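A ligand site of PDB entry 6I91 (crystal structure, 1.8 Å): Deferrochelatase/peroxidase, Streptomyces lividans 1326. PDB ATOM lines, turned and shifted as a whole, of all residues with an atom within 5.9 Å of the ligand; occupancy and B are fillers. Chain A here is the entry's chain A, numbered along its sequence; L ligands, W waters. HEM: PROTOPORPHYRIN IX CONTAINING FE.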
ATOM      1  N   ASN A 179      21.380  10.943 -18.169  1.00  0.00           N
ATOM      2  CA  ASN A 179      21.959   9.986 -17.247  1.00  0.00           C
ATOM      3  C   ASN A 179      22.405   8.733 -18.016  1.00  0.00           C
ATOM      4  O   ASN A 179      22.283   8.641 -19.244  1.00  0.00           O
ATOM      5  CB  ASN A 179      20.979   9.658 -16.110  1.00  0.00           C
ATOM      6  CG  ASN A 179      19.589   9.253 -16.626  1.00  0.00           C
ATOM      7  OD1 ASN A 179      19.477   8.426 -17.532  1.00  0.00           O
ATOM      8  ND2 ASN A 179      18.542   9.828 -16.059  1.00  0.00           N
ATOM      9  N   LEU A 181      21.113   5.853 -18.077  1.00  0.00           N
ATOM     10  CA  LEU A 181      20.020   5.165 -18.761  1.00  0.00           C
ATOM     11  C   LEU A 181      19.686   5.796 -20.107  1.00  0.00           C
ATOM     12  O   LEU A 181      18.837   5.274 -20.832  1.00  0.00           O
ATOM     13  CB  LEU A 181      18.772   5.137 -17.889  1.00  0.00           C
ATOM     14  CG  LEU A 181      18.977   4.490 -16.523  1.00  0.00           C
ATOM     15  CD1 LEU A 181      17.659   4.340 -15.791  1.00  0.00           C
ATOM     16  CD2 LEU A 181      19.673   3.148 -16.691  1.00  0.00           C
ATOM     17  N   PHE A 183      18.370   8.905 -20.731  1.00  0.00           N
ATOM     18  CA  PHE A 183      17.294   9.902 -20.700  1.00  0.00           C
ATOM     19  C   PHE A 183      17.803  11.236 -20.181  1.00  0.00           C
ATOM     20  O   PHE A 183      18.641  11.277 -19.274  1.00  0.00           O
ATOM     21  CB  PHE A 183      16.137   9.420 -19.830  1.00  0.00           C
ATOM     22  CG  PHE A 183      15.242   8.445 -20.523  1.00  0.00           C
ATOM     23  CD1 PHE A 183      15.657   7.134 -20.743  1.00  0.00           C
ATOM     24  CD2 PHE A 183      14.008   8.829 -21.000  1.00  0.00           C
ATOM     25  CE1 PHE A 183      14.854   6.240 -21.405  1.00  0.00           C
ATOM     26  CE2 PHE A 183      13.185   7.933 -21.658  1.00  0.00           C
ATOM     27  CZ  PHE A 183      13.621   6.642 -21.870  1.00  0.00           C
ATOM     28  N   LYS A 184      17.288  12.322 -20.756  1.00  0.00           N
ATOM     29  CA  LYS A 184      17.547  13.656 -20.207  1.00  0.00           C
ATOM     30  C   LYS A 184      17.095  13.691 -18.760  1.00  0.00           C
ATOM     31  O   LYS A 184      16.100  13.071 -18.383  1.00  0.00           O
ATOM     32  CB  LYS A 184      16.828  14.738 -21.015  1.00  0.00           C
ATOM     33  CG  LYS A 184      17.303  14.917 -22.413  1.00  0.00           C
ATOM     34  CD  LYS A 184      16.297  15.712 -23.242  1.00  0.00           C
ATOM     35  CE  LYS A 184      16.910  16.171 -24.555  1.00  0.00           C
ATOM     36  NZ  LYS A 184      15.901  16.917 -25.367  1.00  0.00           N
ATOM     37  N   ASP A 185      17.845  14.405 -17.941  1.00  0.00           N
ATOM     38  CA  ASP A 185      17.609  14.397 -16.505  1.00  0.00           C
ATOM     39  C   ASP A 185      17.765  15.840 -16.058  1.00  0.00           C
ATOM     40  O   ASP A 185      18.871  16.376 -16.138  1.00  0.00           O
ATOM     41  CB  ASP A 185      18.601  13.481 -15.791  1.00  0.00           C
ATOM     42  CG  ASP A 185      18.057  12.856 -14.511  1.00  0.00           C
ATOM     43  OD1 ASP A 185      17.203  13.454 -13.803  1.00  0.00           O
ATOM     44  OD2 ASP A 185      18.516  11.740 -14.211  1.00  0.00           O
ATOM     45  N   GLY A 186      16.674  16.475 -15.622  1.00  0.00           N
ATOM     46  CA  GLY A 186      16.748  17.831 -15.113  1.00  0.00           C
ATOM     47  C   GLY A 186      15.742  18.798 -15.726  1.00  0.00           C
ATOM     48  O   GLY A 186      15.682  19.967 -15.345  1.00  0.00           O
ATOM     49  N   THR A 187      14.925  18.318 -16.666  1.00  0.00           N
ATOM     50  CA  THR A 187      13.981  19.180 -17.369  1.00  0.00           C
ATOM     51  C   THR A 187      13.113  19.981 -16.402  1.00  0.00           C
ATOM     52  O   THR A 187      13.166  21.214 -16.377  1.00  0.00           O
ATOM     53  CB  THR A 187      13.129  18.306 -18.301  1.00  0.00           C
ATOM     54  OG1 THR A 187      14.014  17.537 -19.127  1.00  0.00           O
ATOM     55  CG2 THR A 187      12.170  19.139 -19.182  1.00  0.00           C
ATOM     56  N   ARG A 188      12.335  19.304 -15.565  1.00  0.00           N
ATOM     57  CA  ARG A 188      11.455  19.982 -14.608  1.00  0.00           C
ATOM     58  C   ARG A 188      12.104  19.952 -13.224  1.00  0.00           C
ATOM     59  O   ARG A 188      11.706  19.218 -12.313  1.00  0.00           O
ATOM     60  CB  ARG A 188      10.060  19.363 -14.619  1.00  0.00           C
ATOM     61  CG  ARG A 188       9.192  19.855 -15.787  1.00  0.00           C
ATOM     62  CD  ARG A 188       7.742  19.318 -15.730  1.00  0.00           C
ATOM     63  NE  ARG A 188       7.276  19.224 -14.347  1.00  0.00           N
ATOM     64  CZ  ARG A 188       6.811  20.257 -13.659  1.00  0.00           C
ATOM     65  NH1 ARG A 188       6.439  20.097 -12.393  1.00  0.00           N
ATOM     66  NH2 ARG A 188       6.711  21.445 -14.221  1.00  0.00           N
ATOM     67  N   ASN A 189      13.130  20.775 -13.081  1.00  0.00           N
ATOM     68  CA  ASN A 189      13.794  21.013 -11.805  1.00  0.00           C
ATOM     69  C   ASN A 189      13.421  22.425 -11.347  1.00  0.00           C
ATOM     70  O   ASN A 189      12.422  22.993 -11.805  1.00  0.00           O
ATOM     71  CB  ASN A 189      15.297  20.788 -11.973  1.00  0.00           C
ATOM     72  CG  ASN A 189      15.983  20.499 -10.657  1.00  0.00           C
ATOM     73  OD1 ASN A 189      15.413  19.869  -9.789  1.00  0.00           O
ATOM     74  ND2 ASN A 189      17.224  20.941 -10.532  1.00  0.00           N
ATOM     75  N   ILE A 224      22.705   5.364  -5.724  1.00  0.00           N
ATOM     76  CA  ILE A 224      21.749   4.479  -6.377  1.00  0.00           C
ATOM     77  C   ILE A 224      22.433   3.698  -7.476  1.00  0.00           C
ATOM     78  O   ILE A 224      22.864   4.270  -8.486  1.00  0.00           O
ATOM     79  CB  ILE A 224      20.537   5.254  -6.928  1.00  0.00           C
ATOM     80  CG1 ILE A 224      19.897   6.111  -5.833  1.00  0.00           C
ATOM     81  CG2 ILE A 224      19.510   4.274  -7.516  1.00  0.00           C
ATOM     82  CD1 ILE A 224      18.833   7.107  -6.372  1.00  0.00           C
ATOM     83  N   MET A 226      22.488   1.260 -10.691  1.00  0.00           N
ATOM     84  CA  MET A 226      21.661   0.948 -11.851  1.00  0.00           C
ATOM     85  C   MET A 226      21.960  -0.464 -12.367  1.00  0.00           C
ATOM     86  O   MET A 226      23.136  -0.848 -12.495  1.00  0.00           O
ATOM     87  CB  MET A 226      21.877   1.960 -12.971  1.00  0.00           C
ATOM     88  CG  MET A 226      21.475   3.362 -12.606  1.00  0.00           C
ATOM     89  SD  MET A 226      22.083   4.510 -13.855  1.00  0.00           S
ATOM     90  CE  MET A 226      21.173   5.980 -13.388  1.00  0.00           C
ATOM     91  N   PHE A 243       9.419   5.830 -17.814  1.00  0.00           N
ATOM     92  CA  PHE A 243       9.569   7.226 -17.410  1.00  0.00           C
ATOM     93  C   PHE A 243       8.329   8.060 -17.688  1.00  0.00           C
ATOM     94  O   PHE A 243       7.996   8.933 -16.873  1.00  0.00           O
ATOM     95  CB  PHE A 243      10.782   7.831 -18.115  1.00  0.00           C
ATOM     96  CG  PHE A 243      12.063   7.443 -17.468  1.00  0.00           C
ATOM     97  CD1 PHE A 243      12.354   7.866 -16.178  1.00  0.00           C
ATOM     98  CD2 PHE A 243      12.958   6.631 -18.120  1.00  0.00           C
ATOM     99  CE1 PHE A 243      13.541   7.478 -15.539  1.00  0.00           C
ATOM    100  CE2 PHE A 243      14.144   6.224 -17.494  1.00  0.00           C
ATOM    101  CZ  PHE A 243      14.431   6.665 -16.213  1.00  0.00           C
ATOM    102  N   ARG A 245       8.327   9.763 -20.648  1.00  0.00           N
ATOM    103  CA  ARG A 245       8.865  10.673 -21.647  1.00  0.00           C
ATOM    104  C   ARG A 245       9.514   9.830 -22.740  1.00  0.00           C
ATOM    105  O   ARG A 245       9.946   8.701 -22.474  1.00  0.00           O
ATOM    106  CB  ARG A 245       9.875  11.647 -21.041  1.00  0.00           C
ATOM    107  CG  ARG A 245       9.306  12.657 -20.033  1.00  0.00           C
ATOM    108  CD  ARG A 245      10.388  13.597 -19.583  1.00  0.00           C
ATOM    109  NE  ARG A 245       9.899  14.630 -18.670  1.00  0.00           N
ATOM    110  CZ  ARG A 245       9.501  15.840 -19.034  1.00  0.00           C
ATOM    111  NH1 ARG A 245       9.513  16.195 -20.316  1.00  0.00           N
ATOM    112  NH2 ARG A 245       9.076  16.712 -18.122  1.00  0.00           N
ATOM    113  N   PRO A 262       3.929  18.041 -19.044  1.00  0.00           N
ATOM    114  CA  PRO A 262       3.415  16.680 -19.072  1.00  0.00           C
ATOM    115  C   PRO A 262       1.915  16.660 -18.847  1.00  0.00           C
ATOM    116  O   PRO A 262       1.377  17.476 -18.105  1.00  0.00           O
ATOM    117  CB  PRO A 262       4.181  15.975 -17.940  1.00  0.00           C
ATOM    118  CG  PRO A 262       4.652  17.060 -17.076  1.00  0.00           C
ATOM    119  CD  PRO A 262       4.877  18.260 -17.932  1.00  0.00           C
ATOM    120  N   HIS A 272       7.532   6.926 -13.769  1.00  0.00           N
ATOM    121  CA  HIS A 272       8.348   7.677 -12.819  1.00  0.00           C
ATOM    122  C   HIS A 272       7.930   9.141 -12.743  1.00  0.00           C
ATOM    123  O   HIS A 272       7.749   9.677 -11.647  1.00  0.00           O
ATOM    124  CB  HIS A 272       9.816   7.532 -13.212  1.00  0.00           C
ATOM    125  CG  HIS A 272      10.754   8.181 -12.261  1.00  0.00           C
ATOM    126  ND1 HIS A 272      11.054   7.643 -11.030  1.00  0.00           N
ATOM    127  CD2 HIS A 272      11.484   9.329 -12.369  1.00  0.00           C
ATOM    128  CE1 HIS A 272      11.917   8.428 -10.422  1.00  0.00           C
ATOM    129  NE2 HIS A 272      12.186   9.450 -11.196  1.00  0.00           N
ATOM    130  N   VAL A 273       7.750   9.805 -13.890  1.00  0.00           N
ATOM    131  CA  VAL A 273       7.379  11.222 -13.899  1.00  0.00           C
ATOM    132  C   VAL A 273       6.019  11.424 -13.266  1.00  0.00           C
ATOM    133  O   VAL A 273       5.810  12.358 -12.471  1.00  0.00           O
ATOM    134  CB  VAL A 273       7.405  11.767 -15.326  1.00  0.00           C
ATOM    135  CG1 VAL A 273       6.816  13.149 -15.361  1.00  0.00           C
ATOM    136  CG2 VAL A 273       8.827  11.791 -15.818  1.00  0.00           C
ATOM    137  N   ALA A 276       6.424  11.112  -9.489  1.00  0.00           N
ATOM    138  CA  ALA A 276       7.316  12.085  -8.863  1.00  0.00           C
ATOM    139  C   ALA A 276       6.836  13.519  -8.992  1.00  0.00           C
ATOM    140  O   ALA A 276       7.343  14.391  -8.280  1.00  0.00           O
ATOM    141  CB  ALA A 276       8.714  11.973  -9.472  1.00  0.00           C
ATOM    142  N   HIS A 277       5.854  13.759  -9.835  1.00  0.00           N
ATOM    143  CA  HIS A 277       5.410  15.106 -10.164  1.00  0.00           C
ATOM    144  C   HIS A 277       4.825  15.797  -8.926  1.00  0.00           C
ATOM    145  O   HIS A 277       4.125  15.152  -8.144  1.00  0.00           O
ATOM    146  CB  HIS A 277       4.368  15.017 -11.277  1.00  0.00           C
ATOM    147  CG  HIS A 277       4.097  16.320 -11.969  1.00  0.00           C
ATOM    148  ND1 HIS A 277       3.176  17.228 -11.495  1.00  0.00           N
ATOM    149  CD2 HIS A 277       4.620  16.862 -13.093  1.00  0.00           C
ATOM    150  CE1 HIS A 277       3.149  18.280 -12.295  1.00  0.00           C
ATOM    151  NE2 HIS A 277       4.013  18.081 -13.276  1.00  0.00           N
ATOM    152  N   PRO A 278       5.085  17.085  -8.723  1.00  0.00           N
ATOM    153  CA  PRO A 278       4.505  17.784  -7.560  1.00  0.00           C
ATOM    154  C   PRO A 278       3.007  17.582  -7.395  1.00  0.00           C
ATOM    155  O   PRO A 278       2.522  17.439  -6.271  1.00  0.00           O
ATOM    156  CB  PRO A 278       4.864  19.256  -7.826  1.00  0.00           C
ATOM    157  CG  PRO A 278       6.135  19.191  -8.579  1.00  0.00           C
ATOM    158  CD  PRO A 278       6.100  17.919  -9.398  1.00  0.00           C
ATOM    159  N   LEU A 286      11.309  19.463  -5.352  1.00  0.00           N
ATOM    160  CA  LEU A 286      12.694  19.248  -4.960  1.00  0.00           C
ATOM    161  C   LEU A 286      13.639  19.964  -5.916  1.00  0.00           C
ATOM    162  O   LEU A 286      13.321  20.139  -7.088  1.00  0.00           O
ATOM    163  CB  LEU A 286      13.038  17.748  -4.969  1.00  0.00           C
ATOM    164  CG  LEU A 286      12.155  16.822  -4.148  1.00  0.00           C
ATOM    165  CD1 LEU A 286      12.595  15.388  -4.350  1.00  0.00           C
ATOM    166  CD2 LEU A 286      12.237  17.223  -2.693  1.00  0.00           C
ATOM    167  N   ARG A 288      16.890  18.979  -7.567  1.00  0.00           N
ATOM    168  CA  ARG A 288      17.724  17.829  -7.879  1.00  0.00           C
ATOM    169  C   ARG A 288      19.077  18.313  -8.411  1.00  0.00           C
ATOM    170  O   ARG A 288      19.123  19.181  -9.282  1.00  0.00           O
ATOM    171  CB  ARG A 288      17.022  16.922  -8.886  1.00  0.00           C
ATOM    172  CG  ARG A 288      15.977  15.980  -8.251  1.00  0.00           C
ATOM    173  CD  ARG A 288      15.135  15.216  -9.281  1.00  0.00           C
ATOM    174  NE  ARG A 288      14.442  16.128 -10.181  1.00  0.00           N
ATOM    175  CZ  ARG A 288      14.451  16.041 -11.515  1.00  0.00           C
ATOM    176  NH1 ARG A 288      15.126  15.062 -12.117  1.00  0.00           N
ATOM    177  NH2 ARG A 288      13.779  16.942 -12.227  1.00  0.00           N
ATOM    178  N   LEU A 307      23.787   6.435 -10.107  1.00  0.00           N
ATOM    179  CA  LEU A 307      23.497   7.861 -10.019  1.00  0.00           C
ATOM    180  C   LEU A 307      23.668   8.288  -8.571  1.00  0.00           C
ATOM    181  O   LEU A 307      23.072   7.665  -7.678  1.00  0.00           O
ATOM    182  CB  LEU A 307      22.080   8.160 -10.523  1.00  0.00           C
ATOM    183  CG  LEU A 307      21.649   9.611 -10.704  1.00  0.00           C
ATOM    184  CD1 LEU A 307      20.486   9.690 -11.694  1.00  0.00           C
ATOM    185  CD2 LEU A 307      21.251  10.219  -9.391  1.00  0.00           C
ATOM    186  N   PHE A 309      22.546  10.638  -6.198  1.00  0.00           N
ATOM    187  CA  PHE A 309      21.393  11.510  -6.199  1.00  0.00           C
ATOM    188  C   PHE A 309      21.473  12.499  -5.042  1.00  0.00           C
ATOM    189  O   PHE A 309      21.701  12.109  -3.895  1.00  0.00           O
ATOM    190  CB  PHE A 309      20.123  10.648  -6.151  1.00  0.00           C
ATOM    191  CG  PHE A 309      18.847  11.439  -6.086  1.00  0.00           C
ATOM    192  CD1 PHE A 309      18.317  11.811  -4.862  1.00  0.00           C
ATOM    193  CD2 PHE A 309      18.168  11.760  -7.258  1.00  0.00           C
ATOM    194  CE1 PHE A 309      17.131  12.530  -4.794  1.00  0.00           C
ATOM    195  CE2 PHE A 309      16.975  12.504  -7.203  1.00  0.00           C
ATOM    196  CZ  PHE A 309      16.460  12.879  -5.960  1.00  0.00           C
ATOM    197  N   PHE A 320      11.788  15.293   0.226  1.00  0.00           N
ATOM    198  CA  PHE A 320      12.248  14.000  -0.257  1.00  0.00           C
ATOM    199  C   PHE A 320      11.367  12.859   0.244  1.00  0.00           C
ATOM    200  O   PHE A 320      11.117  11.898  -0.494  1.00  0.00           O
ATOM    201  CB  PHE A 320      13.701  13.747   0.145  1.00  0.00           C
ATOM    202  CG  PHE A 320      14.190  12.407  -0.222  1.00  0.00           C
ATOM    203  CD1 PHE A 320      14.623  12.149  -1.517  1.00  0.00           C
ATOM    204  CD2 PHE A 320      14.199  11.378   0.695  1.00  0.00           C
ATOM    205  CE1 PHE A 320      15.068  10.877  -1.870  1.00  0.00           C
ATOM    206  CE2 PHE A 320      14.634  10.133   0.353  1.00  0.00           C
ATOM    207  CZ  PHE A 320      15.069   9.871  -0.929  1.00  0.00           C
ATOM    208  N   VAL A 323       7.824  12.292  -1.623  1.00  0.00           N
ATOM    209  CA  VAL A 323       8.065  11.879  -3.008  1.00  0.00           C
ATOM    210  C   VAL A 323       8.630  10.461  -3.054  1.00  0.00           C
ATOM    211  O   VAL A 323       8.131   9.611  -3.813  1.00  0.00           O
ATOM    212  CB  VAL A 323       8.980  12.891  -3.743  1.00  0.00           C
ATOM    213  CG1 VAL A 323       9.133  12.490  -5.202  1.00  0.00           C
ATOM    214  CG2 VAL A 323       8.376  14.319  -3.686  1.00  0.00           C
ATOM    215  N   GLN A 324       9.649  10.161  -2.251  1.00  0.00           N
ATOM    216  CA  GLN A 324      10.195   8.800  -2.268  1.00  0.00           C
ATOM    217  C   GLN A 324       9.166   7.784  -1.779  1.00  0.00           C
ATOM    218  O   GLN A 324       9.116   6.655  -2.281  1.00  0.00           O
ATOM    219  CB  GLN A 324      11.485   8.737  -1.447  1.00  0.00           C
ATOM    220  CG  GLN A 324      12.108   7.340  -1.259  1.00  0.00           C
ATOM    221  CD  GLN A 324      12.669   6.717  -2.532  1.00  0.00           C
ATOM    222  OE1 GLN A 324      13.012   7.396  -3.483  1.00  0.00           O
ATOM    223  NE2 GLN A 324      12.782   5.402  -2.538  1.00  0.00           N
ATOM    224  N   LEU A 327       7.158   6.726  -4.586  1.00  0.00           N
ATOM    225  CA  LEU A 327       7.832   5.919  -5.599  1.00  0.00           C
ATOM    226  C   LEU A 327       7.853   4.435  -5.238  1.00  0.00           C
ATOM    227  O   LEU A 327       8.562   3.660  -5.881  1.00  0.00           O
ATOM    228  CB  LEU A 327       9.257   6.426  -5.831  1.00  0.00           C
ATOM    229  CG  LEU A 327       9.387   7.910  -6.205  1.00  0.00           C
ATOM    230  CD1 LEU A 327      10.833   8.306  -6.482  1.00  0.00           C
ATOM    231  CD2 LEU A 327       8.495   8.256  -7.402  1.00  0.00           C
ATOM    232  N   LEU A 332      10.478   2.313 -12.330  1.00  0.00           N
ATOM    233  CA  LEU A 332      11.929   2.384 -12.332  1.00  0.00           C
ATOM    234  C   LEU A 332      12.572   1.472 -11.284  1.00  0.00           C
ATOM    235  O   LEU A 332      13.742   1.128 -11.422  1.00  0.00           O
ATOM    236  CB  LEU A 332      12.371   3.825 -12.083  1.00  0.00           C
ATOM    237  CG  LEU A 332      13.850   4.162 -12.181  1.00  0.00           C
ATOM    238  CD1 LEU A 332      14.376   3.798 -13.560  1.00  0.00           C
ATOM    239  CD2 LEU A 332      14.042   5.648 -11.928  1.00  0.00           C
ATOM    240  N   ILE A 336      16.919  -0.242 -10.417  1.00  0.00           N
ATOM    241  CA  ILE A 336      17.792   0.546  -9.569  1.00  0.00           C
ATOM    242  C   ILE A 336      17.744  -0.024  -8.158  1.00  0.00           C
ATOM    243  O   ILE A 336      16.850  -0.784  -7.801  1.00  0.00           O
ATOM    244  CB  ILE A 336      17.421   2.049  -9.545  1.00  0.00           C
ATOM    245  CG1 ILE A 336      16.002   2.239  -9.000  1.00  0.00           C
ATOM    246  CG2 ILE A 336      17.521   2.647 -10.944  1.00  0.00           C
ATOM    247  CD1 ILE A 336      15.719   3.643  -8.459  1.00  0.00           C
ATOM    248  N   HIS A 338      18.849   1.503  -4.109  1.00  0.00           N
ATOM    249  CA  HIS A 338      19.498   2.469  -3.231  1.00  0.00           C
ATOM    250  C   HIS A 338      20.449   1.731  -2.297  1.00  0.00           C
ATOM    251  O   HIS A 338      20.038   0.768  -1.638  1.00  0.00           O
ATOM    252  CB  HIS A 338      18.466   3.251  -2.411  1.00  0.00           C
ATOM    253  CG  HIS A 338      17.539   4.085  -3.240  1.00  0.00           C
ATOM    254  ND1 HIS A 338      17.407   5.452  -3.064  1.00  0.00           N
ATOM    255  CD2 HIS A 338      16.679   3.756  -4.224  1.00  0.00           C
ATOM    256  CE1 HIS A 338      16.524   5.921  -3.926  1.00  0.00           C
ATOM    257  NE2 HIS A 338      16.068   4.905  -4.645  1.00  0.00           N
HETATM  258  CHA HEM L   1      12.150  13.436 -13.248  1.00  0.00           C
HETATM  259  CHB HEM L   1      15.408   9.880 -13.852  1.00  0.00           C
HETATM  260  CHC HEM L   1      15.558   9.043  -9.085  1.00  0.00           C
HETATM  261  CHD HEM L   1      12.417  12.684  -8.431  1.00  0.00           C
HETATM  262  C1A HEM L   1      13.005  12.532 -13.841  1.00  0.00           C
HETATM  263  C2A HEM L   1      13.210  12.349 -15.257  1.00  0.00           C
HETATM  264  C3A HEM L   1      14.096  11.358 -15.400  1.00  0.00           C
HETATM  265  C4A HEM L   1      14.497  10.884 -14.107  1.00  0.00           C
HETATM  266  CMA HEM L   1      14.669  10.753 -16.708  1.00  0.00           C
HETATM  267  CAA HEM L   1      12.490  13.167 -16.367  1.00  0.00           C
HETATM  268  CBA HEM L   1      13.180  14.525 -16.669  1.00  0.00           C
HETATM  269  CGA HEM L   1      13.166  15.553 -15.554  1.00  0.00           C
HETATM  270  O1A HEM L   1      12.132  16.257 -15.398  1.00  0.00           O
HETATM  271  O2A HEM L   1      14.172  15.708 -14.821  1.00  0.00           O
HETATM  272  C1B HEM L   1      15.747   9.358 -12.626  1.00  0.00           C
HETATM  273  C2B HEM L   1      16.702   8.299 -12.382  1.00  0.00           C
HETATM  274  C3B HEM L   1      16.731   8.043 -11.058  1.00  0.00           C
HETATM  275  C4B HEM L   1      15.811   8.965 -10.429  1.00  0.00           C
HETATM  276  CMB HEM L   1      17.513   7.588 -13.483  1.00  0.00           C
HETATM  277  CAB HEM L   1      17.609   7.028 -10.292  1.00  0.00           C
HETATM  278  CBB HEM L   1      18.631   6.418 -10.894  1.00  0.00           C
HETATM  279  C1C HEM L   1      14.720   9.966  -8.505  1.00  0.00           C
HETATM  280  C2C HEM L   1      14.428  10.055  -7.103  1.00  0.00           C
HETATM  281  C3C HEM L   1      13.560  11.063  -6.914  1.00  0.00           C
HETATM  282  C4C HEM L   1      13.274  11.628  -8.208  1.00  0.00           C
HETATM  283  CMC HEM L   1      15.110   9.106  -6.075  1.00  0.00           C
HETATM  284  CAC HEM L   1      12.917  11.598  -5.625  1.00  0.00           C
HETATM  285  CBC HEM L   1      12.996  10.897  -4.487  1.00  0.00           C
HETATM  286  C1D HEM L   1      12.115  13.217  -9.670  1.00  0.00           C
HETATM  287  C2D HEM L   1      11.329  14.392  -9.891  1.00  0.00           C
HETATM  288  C3D HEM L   1      11.236  14.610 -11.195  1.00  0.00           C
HETATM  289  C4D HEM L   1      11.979  13.577 -11.883  1.00  0.00           C
HETATM  290  CMD HEM L   1      10.691  15.214  -8.754  1.00  0.00           C
HETATM  291  CAD HEM L   1      10.469  15.769 -11.863  1.00  0.00           C
HETATM  292  CBD HEM L   1       9.097  15.279 -12.288  1.00  0.00           C
HETATM  293  CGD HEM L   1       8.272  16.467 -12.684  1.00  0.00           C
HETATM  294  O1D HEM L   1       7.877  16.549 -13.873  1.00  0.00           O
HETATM  295  O2D HEM L   1       8.072  17.358 -11.821  1.00  0.00           O
HETATM  296  NA  HEM L   1      13.793  11.610 -13.170  1.00  0.00           N
HETATM  297  NB  HEM L   1      15.223   9.730 -11.427  1.00  0.00           N
HETATM  298  NC  HEM L   1      13.983  10.930  -9.161  1.00  0.00           N
HETATM  299  ND  HEM L   1      12.506  12.750 -10.910  1.00  0.00           N
HETATM  300 FE   HEM L   1      13.742  11.142 -11.156  1.00  0.00          FE
HETATM  301  O   HOH W   1      10.209  18.433  -7.930  1.00  0.00           O
HETATM  302  O   HOH W   2       9.532  15.531 -15.997  1.00  0.00           O
HETATM  303  O   HOH W   3       9.523  19.107 -10.380  1.00  0.00           O
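O of Arg 188 lies within hydrogen-bond range of NH2 of Arg 288 (3.1 Å). A ring nitrogen (NE2) of His 277 sits at hydrogen-bond distance from the guanidinium group (NH1) of Arg 188 (3.3 Å). The backbone NH (N) of Arg 288 sits at hydrogen-bond distance from the side-chain amide oxygen (OD1) of Asn 189 (2.8 Å). The backbone NH of Val 273 sits at hydrogen-bond distance from the backbone carbonyl oxygen of Phe 243 (3.1 Å). The side-chain amide nitrogen (ND2) of Asn 179 is in hydrogen-bond range of the side-chain carboxylate (OD2) of Asp 185 (2.7 Å). OD1 of Asn 179 lies within hydrogen-bond range of N of Phe 183 (3.4 Å). The side-chain amide oxygen of Asn 179 is in hydrogen-bond range of the backbone NH of Leu 181, 3.1 Å away. The backbone NH (N) of Leu 307 lies within hydrogen-bond range of the backbone carbonyl oxygen (O) of Ile 224, 2.9 Å away.
NE2 of His 272 is bound to FE of the ligand, 2.3 Å away. The backbone NH (N) of Gly 186 sits at hydrogen-bond distance from an oxygen (O2A) of the ligand, 2.7 Å away. An oxygen (O1A) of the ligand sits at hydrogen-bond distance from the backbone NH (N) of Arg 188 (3.1 Å). NE of Arg 188 is in salt-bridge range of O1D of the ligand. The guanidinium group (NH2) of Arg 288 is in salt-bridge range of an oxygen (O2A) of the ligand (2.9 Å). The backbone NH (N) of Thr 187 sits at hydrogen-bond distance from an oxygen (O2A) of the ligand (3.3 Å).
Merely in contact with the ligand: Asn 179 (3.6 Å), Leu 181 (3.99 Å), Phe 183 (3.7 Å), Lys 184 (3.2 Å), Asp 185 (3.6 Å), Met 226 (3.6 Å), Phe 243 (3.5 Å), Arg 245 (3.8 Å), Val 273 (3.9 Å), Ala 276 (3.5 Å), His 277 (3.4 Å), Pro 278 (3.2 Å), Leu 307 (3.8 Å), Phe 309 (3.5 Å), Phe 320 (3.3 Å), Val 323 (3.9 Å), Gln 324 (3.6 Å), Leu 327 (3.9 Å), Leu 332 (3.7 Å) and Ile 336 (3.9 Å). Hydrophobic or aromatic side chains within 4 Å of the ligand: Leu 181, Phe 183, Met 226, Phe 243, His 272, Val 273, Ala 276, His 277, Pro 278, Leu 307, Phe 309, Phe 320, Val 323, Leu 327, Leu 332 and Ile 336. 25 residues have an atom within 4 Å of the ligand: Asn 179, Leu 181, Phe 183, Lys 184, Asp 185, Gly 186, Thr 187, Arg 188, Met 226, Phe 243, Arg 245, His 272, Val 273, Ala 276, His 277, Pro 278, Arg 288, Leu 307, Phe 309, Phe 320, Val 323, Gln 324, Leu 327, Leu 332 and Ile 336. The nearest printed residue that does not touch the ligand is Leu 286 (4.01 Å).
Water W3 lies within hydrogen-bond range of O2D of the ligand and O of Arg 188. Water W2 bridges NH2 of Arg 245 (2.5 Å) and O1A of the ligand (2.8 Å).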
